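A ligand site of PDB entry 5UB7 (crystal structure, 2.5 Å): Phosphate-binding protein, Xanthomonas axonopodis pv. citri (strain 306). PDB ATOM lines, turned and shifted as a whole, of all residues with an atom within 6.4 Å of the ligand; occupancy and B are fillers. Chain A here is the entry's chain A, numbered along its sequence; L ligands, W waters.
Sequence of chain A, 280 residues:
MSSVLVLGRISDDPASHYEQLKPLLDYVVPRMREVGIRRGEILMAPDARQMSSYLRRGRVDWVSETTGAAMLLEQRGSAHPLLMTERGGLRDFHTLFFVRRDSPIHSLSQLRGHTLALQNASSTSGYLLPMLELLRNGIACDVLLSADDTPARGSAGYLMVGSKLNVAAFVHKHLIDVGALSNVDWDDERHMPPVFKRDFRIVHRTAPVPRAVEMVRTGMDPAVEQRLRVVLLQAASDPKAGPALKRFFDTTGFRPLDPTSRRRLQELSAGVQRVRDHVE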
ATOM      1  N   ARG A   9       6.895  10.353  13.217  1.00  0.00           N
ATOM      2  CA  ARG A   9       8.168  11.079  13.235  1.00  0.00           C
ATOM      3  C   ARG A   9       8.067  12.339  14.071  1.00  0.00           C
ATOM      4  O   ARG A   9       6.966  12.768  14.403  1.00  0.00           O
ATOM      5  CB  ARG A   9       8.618  11.449  11.819  1.00  0.00           C
ATOM      6  CG  ARG A   9       7.703  12.430  11.080  1.00  0.00           C
ATOM      7  CD  ARG A   9       8.417  12.984   9.870  1.00  0.00           C
ATOM      8  NE  ARG A   9       9.167  14.173  10.192  1.00  0.00           N
ATOM      9  CZ  ARG A   9      10.127  14.709   9.436  1.00  0.00           C
ATOM     10  NH1 ARG A   9      10.494  14.155   8.271  1.00  0.00           N
ATOM     11  NH2 ARG A   9      10.749  15.804   9.870  1.00  0.00           N
ATOM     12  N   ILE A  10       9.227  12.930  14.352  1.00  0.00           N
ATOM     13  CA  ILE A  10       9.294  14.206  15.023  1.00  0.00           C
ATOM     14  C   ILE A  10       8.906  15.231  13.975  1.00  0.00           C
ATOM     15  O   ILE A  10       9.511  15.259  12.923  1.00  0.00           O
ATOM     16  CB  ILE A  10      10.678  14.547  15.535  1.00  0.00           C
ATOM     17  CG1 ILE A  10      11.175  13.455  16.481  1.00  0.00           C
ATOM     18  CG2 ILE A  10      10.652  15.885  16.260  1.00  0.00           C
ATOM     19  CD1 ILE A  10      12.661  13.583  16.762  1.00  0.00           C
ATOM     20  N   HIS A  17       3.205  16.266   7.176  1.00  0.00           N
ATOM     21  CA  HIS A  17       3.884  14.988   7.376  1.00  0.00           C
ATOM     22  C   HIS A  17       2.929  13.794   7.479  1.00  0.00           C
ATOM     23  O   HIS A  17       3.293  12.693   7.048  1.00  0.00           O
ATOM     24  CB  HIS A  17       4.892  15.078   8.534  1.00  0.00           C
ATOM     25  CG  HIS A  17       6.104  15.921   8.229  1.00  0.00           C
ATOM     26  ND1 HIS A  17       6.739  15.897   7.003  1.00  0.00           N
ATOM     27  CD2 HIS A  17       6.804  16.785   8.996  1.00  0.00           C
ATOM     28  CE1 HIS A  17       7.776  16.712   7.034  1.00  0.00           C
ATOM     29  NE2 HIS A  17       7.841  17.265   8.236  1.00  0.00           N
ATOM     30  N   GLN A  20       2.373  12.120   4.180  1.00  0.00           N
ATOM     31  CA  GLN A  20       3.600  11.464   3.793  1.00  0.00           C
ATOM     32  C   GLN A  20       3.772  10.081   4.461  1.00  0.00           C
ATOM     33  O   GLN A  20       4.465   9.221   3.895  1.00  0.00           O
ATOM     34  CB  GLN A  20       4.789  12.391   4.044  1.00  0.00           C
ATOM     35  CG  GLN A  20       4.747  13.638   3.157  1.00  0.00           C
ATOM     36  CD  GLN A  20       6.091  14.338   3.091  1.00  0.00           C
ATOM     37  OE1 GLN A  20       6.369  15.213   3.905  1.00  0.00           O
ATOM     38  NE2 GLN A  20       6.955  13.912   2.162  1.00  0.00           N
ATOM     39  N   GLU A  65      13.501   8.823  10.378  1.00  0.00           N
ATOM     40  CA  GLU A  65      14.156  10.056  10.822  1.00  0.00           C
ATOM     41  C   GLU A  65      15.473  10.272  10.108  1.00  0.00           C
ATOM     42  O   GLU A  65      16.139   9.320   9.731  1.00  0.00           O
ATOM     43  CB  GLU A  65      14.486   9.990  12.334  1.00  0.00           C
ATOM     44  CG  GLU A  65      13.310  10.068  13.266  1.00  0.00           C
ATOM     45  CD  GLU A  65      12.599  11.394  13.188  1.00  0.00           C
ATOM     46  OE1 GLU A  65      13.238  12.378  12.798  1.00  0.00           O
ATOM     47  OE2 GLU A  65      11.397  11.458  13.524  1.00  0.00           O
ATOM     48  N   THR A  66      15.876  11.534  10.006  1.00  0.00           N
ATOM     49  CA  THR A  66      17.238  11.832   9.665  1.00  0.00           C
ATOM     50  C   THR A  66      18.063  11.342  10.821  1.00  0.00           C
ATOM     51  O   THR A  66      17.561  11.135  11.941  1.00  0.00           O
ATOM     52  CB  THR A  66      17.443  13.303   9.402  1.00  0.00           C
ATOM     53  OG1 THR A  66      16.932  14.040  10.503  1.00  0.00           O
ATOM     54  CG2 THR A  66      16.694  13.698   8.145  1.00  0.00           C
ATOM     55  N   THR A  67      19.332  11.116  10.528  1.00  0.00           N
ATOM     56  CA  THR A  67      20.179  10.337  11.391  1.00  0.00           C
ATOM     57  C   THR A  67      20.541  11.033  12.687  1.00  0.00           C
ATOM     58  O   THR A  67      20.513  10.372  13.710  1.00  0.00           O
ATOM     59  CB  THR A  67      21.414   9.807  10.632  1.00  0.00           C
ATOM     60  OG1 THR A  67      22.088  10.888   9.932  1.00  0.00           O
ATOM     61  CG2 THR A  67      20.935   8.772   9.616  1.00  0.00           C
ATOM     62  N   ALA A  69      18.552  13.239  14.327  1.00  0.00           N
ATOM     63  CA  ALA A  69      17.345  13.114  15.120  1.00  0.00           C
ATOM     64  C   ALA A  69      17.211  11.706  15.635  1.00  0.00           C
ATOM     65  O   ALA A  69      16.836  11.484  16.784  1.00  0.00           O
ATOM     66  CB  ALA A  69      16.128  13.472  14.325  1.00  0.00           C
ATOM     67  N   ARG A  87      16.987   8.499   0.394  1.00  0.00           N
ATOM     68  CA  ARG A  87      15.938   9.433  -0.026  1.00  0.00           C
ATOM     69  C   ARG A  87      16.377  10.264  -1.239  1.00  0.00           C
ATOM     70  O   ARG A  87      17.514  10.757  -1.289  1.00  0.00           O
ATOM     71  CB  ARG A  87      15.593  10.380   1.135  1.00  0.00           C
ATOM     72  CG  ARG A  87      14.764   9.711   2.213  1.00  0.00           C
ATOM     73  CD  ARG A  87      14.535  10.670   3.362  1.00  0.00           C
ATOM     74  NE  ARG A  87      13.838  10.019   4.453  1.00  0.00           N
ATOM     75  CZ  ARG A  87      13.479  10.606   5.591  1.00  0.00           C
ATOM     76  NH1 ARG A  87      13.733  11.890   5.825  1.00  0.00           N
ATOM     77  NH2 ARG A  87      12.851   9.889   6.512  1.00  0.00           N
ATOM     78  N   PHE A  93      23.878  12.884   3.134  1.00  0.00           N
ATOM     79  CA  PHE A  93      23.737  14.301   2.902  1.00  0.00           C
ATOM     80  C   PHE A  93      24.666  15.054   3.836  1.00  0.00           C
ATOM     81  O   PHE A  93      25.404  14.450   4.671  1.00  0.00           O
ATOM     82  CB  PHE A  93      22.262  14.764   2.903  1.00  0.00           C
ATOM     83  CG  PHE A  93      21.588  14.906   4.268  1.00  0.00           C
ATOM     84  CD1 PHE A  93      21.988  14.194   5.394  1.00  0.00           C
ATOM     85  CD2 PHE A  93      20.472  15.738   4.377  1.00  0.00           C
ATOM     86  CE1 PHE A  93      21.342  14.364   6.593  1.00  0.00           C
ATOM     87  CE2 PHE A  93      19.804  15.891   5.572  1.00  0.00           C
ATOM     88  CZ  PHE A  93      20.248  15.197   6.685  1.00  0.00           C
ATOM     89  N   GLN A 119      17.367  25.901  12.508  1.00  0.00           N
ATOM     90  CA  GLN A 119      16.007  25.431  12.362  1.00  0.00           C
ATOM     91  C   GLN A 119      15.320  25.131  13.707  1.00  0.00           C
ATOM     92  O   GLN A 119      14.591  25.970  14.225  1.00  0.00           O
ATOM     93  CB  GLN A 119      15.964  24.251  11.390  1.00  0.00           C
ATOM     94  CG  GLN A 119      15.986  24.773   9.954  1.00  0.00           C
ATOM     95  CD  GLN A 119      16.498  23.764   8.925  1.00  0.00           C
ATOM     96  OE1 GLN A 119      15.934  22.693   8.737  1.00  0.00           O
ATOM     97  NE2 GLN A 119      17.566  24.142   8.220  1.00  0.00           N
ATOM     98  N   ASN A 120      15.543  23.961  14.255  1.00  0.00           N
ATOM     99  CA  ASN A 120      14.920  23.547  15.495  1.00  0.00           C
ATOM    100  C   ASN A 120      15.787  22.431  16.049  1.00  0.00           C
ATOM    101  O   ASN A 120      16.541  21.800  15.304  1.00  0.00           O
ATOM    102  CB  ASN A 120      13.471  23.113  15.288  1.00  0.00           C
ATOM    103  CG  ASN A 120      13.334  21.760  14.556  1.00  0.00           C
ATOM    104  OD1 ASN A 120      13.416  20.677  15.152  1.00  0.00           O
ATOM    105  ND2 ASN A 120      13.097  21.842  13.255  1.00  0.00           N
ATOM    106  N   SER A 122      15.618  19.406  16.817  1.00  0.00           N
ATOM    107  CA  SER A 122      15.586  18.061  16.276  1.00  0.00           C
ATOM    108  C   SER A 122      16.141  17.949  14.834  1.00  0.00           C
ATOM    109  O   SER A 122      16.200  16.834  14.322  1.00  0.00           O
ATOM    110  CB  SER A 122      14.152  17.553  16.328  1.00  0.00           C
ATOM    111  OG  SER A 122      13.590  17.702  17.631  1.00  0.00           O
ATOM    112  N   SER A 123      16.524  19.056  14.203  1.00  0.00           N
ATOM    113  CA  SER A 123      16.984  19.031  12.786  1.00  0.00           C
ATOM    114  C   SER A 123      18.431  18.571  12.699  1.00  0.00           C
ATOM    115  O   SER A 123      19.339  19.128  13.353  1.00  0.00           O
ATOM    116  CB  SER A 123      16.867  20.415  12.157  1.00  0.00           C
ATOM    117  OG  SER A 123      17.310  20.441  10.824  1.00  0.00           O
ATOM    118  N   THR A 124      18.629  17.519  11.911  1.00  0.00           N
ATOM    119  CA  THR A 124      19.960  16.988  11.666  1.00  0.00           C
ATOM    120  C   THR A 124      20.779  18.010  10.840  1.00  0.00           C
ATOM    121  O   THR A 124      21.857  18.419  11.270  1.00  0.00           O
ATOM    122  CB  THR A 124      19.861  15.621  10.939  1.00  0.00           C
ATOM    123  OG1 THR A 124      19.272  14.623  11.804  1.00  0.00           O
ATOM    124  CG2 THR A 124      21.197  15.154  10.498  1.00  0.00           C
ATOM    125  N   SER A 125      20.279  18.420   9.696  1.00  0.00           N
ATOM    126  CA  SER A 125      21.024  19.315   8.803  1.00  0.00           C
ATOM    127  C   SER A 125      20.945  20.795   9.159  1.00  0.00           C
ATOM    128  O   SER A 125      21.803  21.602   8.743  1.00  0.00           O
ATOM    129  CB  SER A 125      20.579  19.142   7.349  1.00  0.00           C
ATOM    130  OG  SER A 125      19.256  19.597   7.138  1.00  0.00           O
ATOM    131  N   GLY A 126      19.928  21.164   9.914  1.00  0.00           N
ATOM    132  CA  GLY A 126      19.693  22.579  10.258  1.00  0.00           C
ATOM    133  C   GLY A 126      19.961  22.973  11.689  1.00  0.00           C
ATOM    134  O   GLY A 126      19.700  24.102  12.068  1.00  0.00           O
ATOM    135  N   LYS A 164      12.855  25.746   7.273  1.00  0.00           N
ATOM    136  CA  LYS A 164      13.861  25.847   6.242  1.00  0.00           C
ATOM    137  C   LYS A 164      13.733  27.126   5.406  1.00  0.00           C
ATOM    138  O   LYS A 164      14.768  27.787   5.134  1.00  0.00           O
ATOM    139  CB  LYS A 164      13.844  24.600   5.388  1.00  0.00           C
ATOM    140  CG  LYS A 164      14.450  23.447   6.171  1.00  0.00           C
ATOM    141  CD  LYS A 164      14.290  22.069   5.575  1.00  0.00           C
ATOM    142  CE  LYS A 164      15.049  21.109   6.496  1.00  0.00           C
ATOM    143  NZ  LYS A 164      15.195  19.745   5.970  1.00  0.00           N
ATOM    144  N   SER A 182      20.747  21.768   4.499  1.00  0.00           N
ATOM    145  CA  SER A 182      21.340  20.595   3.841  1.00  0.00           C
ATOM    146  C   SER A 182      21.678  20.862   2.356  1.00  0.00           C
ATOM    147  O   SER A 182      21.105  21.742   1.701  1.00  0.00           O
ATOM    148  CB  SER A 182      20.435  19.387   3.941  1.00  0.00           C
ATOM    149  OG  SER A 182      19.515  19.389   2.868  1.00  0.00           O
ATOM    150  N   VAL A 184      20.729  18.994  -0.008  1.00  0.00           N
ATOM    151  CA  VAL A 184      19.466  18.650  -0.654  1.00  0.00           C
ATOM    152  C   VAL A 184      18.521  19.841  -0.621  1.00  0.00           C
ATOM    153  O   VAL A 184      17.858  20.165  -1.617  1.00  0.00           O
ATOM    154  CB  VAL A 184      18.800  17.439   0.033  1.00  0.00           C
ATOM    155  CG1 VAL A 184      17.390  17.194  -0.503  1.00  0.00           C
ATOM    156  CG2 VAL A 184      19.661  16.193  -0.152  1.00  0.00           C
ATOM    157  N   ASP A 185      18.455  20.468   0.558  1.00  0.00           N
ATOM    158  CA  ASP A 185      17.671  21.686   0.752  1.00  0.00           C
ATOM    159  C   ASP A 185      18.051  22.794  -0.205  1.00  0.00           C
ATOM    160  O   ASP A 185      17.186  23.558  -0.614  1.00  0.00           O
ATOM    161  CB  ASP A 185      17.844  22.212   2.172  1.00  0.00           C
ATOM    162  CG  ASP A 185      17.034  21.458   3.193  1.00  0.00           C
ATOM    163  OD1 ASP A 185      15.977  20.912   2.802  1.00  0.00           O
ATOM    164  OD2 ASP A 185      17.428  21.475   4.398  1.00  0.00           O
ATOM    165  N   HIS A 191      12.198  25.506  -0.395  1.00  0.00           N
ATOM    166  CA  HIS A 191      12.977  26.013   0.752  1.00  0.00           C
ATOM    167  C   HIS A 191      14.123  26.947   0.406  1.00  0.00           C
ATOM    168  O   HIS A 191      14.531  27.765   1.264  1.00  0.00           O
ATOM    169  CB  HIS A 191      13.515  24.860   1.586  1.00  0.00           C
ATOM    170  CG  HIS A 191      12.457  23.869   1.919  1.00  0.00           C
ATOM    171  ND1 HIS A 191      12.522  22.561   1.499  1.00  0.00           N
ATOM    172  CD2 HIS A 191      11.273  24.017   2.542  1.00  0.00           C
ATOM    173  CE1 HIS A 191      11.435  21.941   1.879  1.00  0.00           C
ATOM    174  NE2 HIS A 191      10.659  22.798   2.523  1.00  0.00           N
ATOM    175  N   ARG A 211      21.780   9.676   5.349  1.00  0.00           N
ATOM    176  CA  ARG A 211      20.637  10.553   5.041  1.00  0.00           C
ATOM    177  C   ARG A 211      19.460  10.374   6.005  1.00  0.00           C
ATOM    178  O   ARG A 211      18.804  11.351   6.336  1.00  0.00           O
ATOM    179  CB  ARG A 211      20.222  10.266   3.578  1.00  0.00           C
ATOM    180  CG  ARG A 211      18.998  10.970   3.014  1.00  0.00           C
ATOM    181  CD  ARG A 211      19.309  12.369   2.526  1.00  0.00           C
ATOM    182  NE  ARG A 211      18.101  13.128   2.235  1.00  0.00           N
ATOM    183  CZ  ARG A 211      17.269  13.625   3.136  1.00  0.00           C
ATOM    184  NH1 ARG A 211      17.462  13.443   4.460  1.00  0.00           N
ATOM    185  NH2 ARG A 211      16.192  14.297   2.723  1.00  0.00           N
ATOM    186  N   ALA A 212      19.231   9.142   6.474  1.00  0.00           N
ATOM    187  CA  ALA A 212      18.020   8.748   7.236  1.00  0.00           C
ATOM    188  C   ALA A 212      18.084   7.291   7.686  1.00  0.00           C
ATOM    189  O   ALA A 212      18.884   6.519   7.147  1.00  0.00           O
ATOM    190  CB  ALA A 212      16.761   8.952   6.407  1.00  0.00           C
ATOM    191  N   PHE A 249       8.556  10.768   1.997  1.00  0.00           N
ATOM    192  CA  PHE A 249       9.766  11.604   1.904  1.00  0.00           C
ATOM    193  C   PHE A 249      10.668  11.196   0.729  1.00  0.00           C
ATOM    194  O   PHE A 249      11.883  11.271   0.818  1.00  0.00           O
ATOM    195  CB  PHE A 249      10.544  11.573   3.226  1.00  0.00           C
ATOM    196  CG  PHE A 249       9.671  11.566   4.462  1.00  0.00           C
ATOM    197  CD1 PHE A 249       9.056  12.726   4.921  1.00  0.00           C
ATOM    198  CD2 PHE A 249       9.479  10.389   5.197  1.00  0.00           C
ATOM    199  CE1 PHE A 249       8.258  12.715   6.056  1.00  0.00           C
ATOM    200  CE2 PHE A 249       8.670  10.369   6.330  1.00  0.00           C
ATOM    201  CZ  PHE A 249       8.069  11.540   6.772  1.00  0.00           C
HETATM  202  P1  LIG L   1      16.561  17.491   8.810  1.00  0.00           P
HETATM  203  O1  LIG L   1      16.272  16.590   9.988  1.00  0.00           O
HETATM  204  O2  LIG L   1      18.011  17.428   8.371  1.00  0.00           O
HETATM  205  O3  LIG L   1      16.044  18.918   8.998  1.00  0.00           O
HETATM  206  P2  LIG L   1      14.166  16.631   7.407  1.00  0.00           P
HETATM  207  O4  LIG L   1      13.501  16.027   8.661  1.00  0.00           O
HETATM  208  O5  LIG L   1      13.500  17.830   6.783  1.00  0.00           O
HETATM  209  O6  LIG L   1      15.759  16.925   7.499  1.00  0.00           O
HETATM  210  P3  LIG L   1      13.306  15.285   5.023  1.00  0.00           P
HETATM  211  O7  LIG L   1      13.748  13.962   4.448  1.00  0.00           O
HETATM  212  O8  LIG L   1      11.869  15.514   5.493  1.00  0.00           O
HETATM  213  O9  LIG L   1      14.271  15.443   6.315  1.00  0.00           O
HETATM  214  O10 LIG L   1      13.826  16.423   3.969  1.00  0.00           O
HETATM  215  O   HOH W   1      13.967  17.366  12.194  1.00  0.00           O
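CZ of Phe 93 touches O2 of the ligand, 3.6 Å away.
OE1 of Gln 119 touches O3 of the ligand, at 3.8 Å.
Hydrophobic or aromatic side chains within 4 Å of the ligand: Phe 93.
Of the 25 residues printed, 10 come within 4 Å of the ligand.
NZ of Lys 164 lies within salt-bridge range of OD2 of Asp 185 (3.2 Å).
OG1 of Thr 66 sits at hydrogen-bond distance from OG1 of Thr 124, 2.7 Å away.
The side-chain amide oxygen of Gln 119 lies within hydrogen-bond range of the side-chain hydroxyl of Ser 123, at 3.4 Å.
OG of Ser 123 lies within hydrogen-bond range of N of Gly 126 (2.9 Å).
The side-chain hydroxyl (OG1) of Thr 124 sits at hydrogen-bond distance from the backbone NH (N) of Ala 69, 3.0 Å away.
The backbone NH of Gln 119 is in hydrogen-bond range of the backbone carbonyl oxygen of Gly 126 (3.0 Å).
Water W1 bridges O of Ser 122 and O1 of the ligand.
NH1 of Arg 87 lies within salt-bridge range of O7 of the ligand, 2.5 Å away.
An oxygen (O5) of the ligand lies within salt-bridge range of the side-chain amino group (NZ) of Lys 164 (2.7 Å).
OG1 of Thr 66 is in hydrogen-bond range of O1 of the ligand (2.7 Å).
OG of Ser 123 lies within hydrogen-bond range of O3 of the ligand (2.7 Å).
N of Ser 125 sits at hydrogen-bond distance from O2 of the ligand, at 2.8 Å.
OG of Ser 125 sits at hydrogen-bond distance from O2 of the ligand (2.8 Å).
NH2 of Arg 211 lies within salt-bridge range of O7 of the ligand, 3.0 Å away.
The guanidinium group (NH2) of Arg 9 is in salt-bridge range of an oxygen (O4) of the ligand (3.0 Å).
N of Thr 124 lies within hydrogen-bond range of O1 of the ligand, at 3.2 Å.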
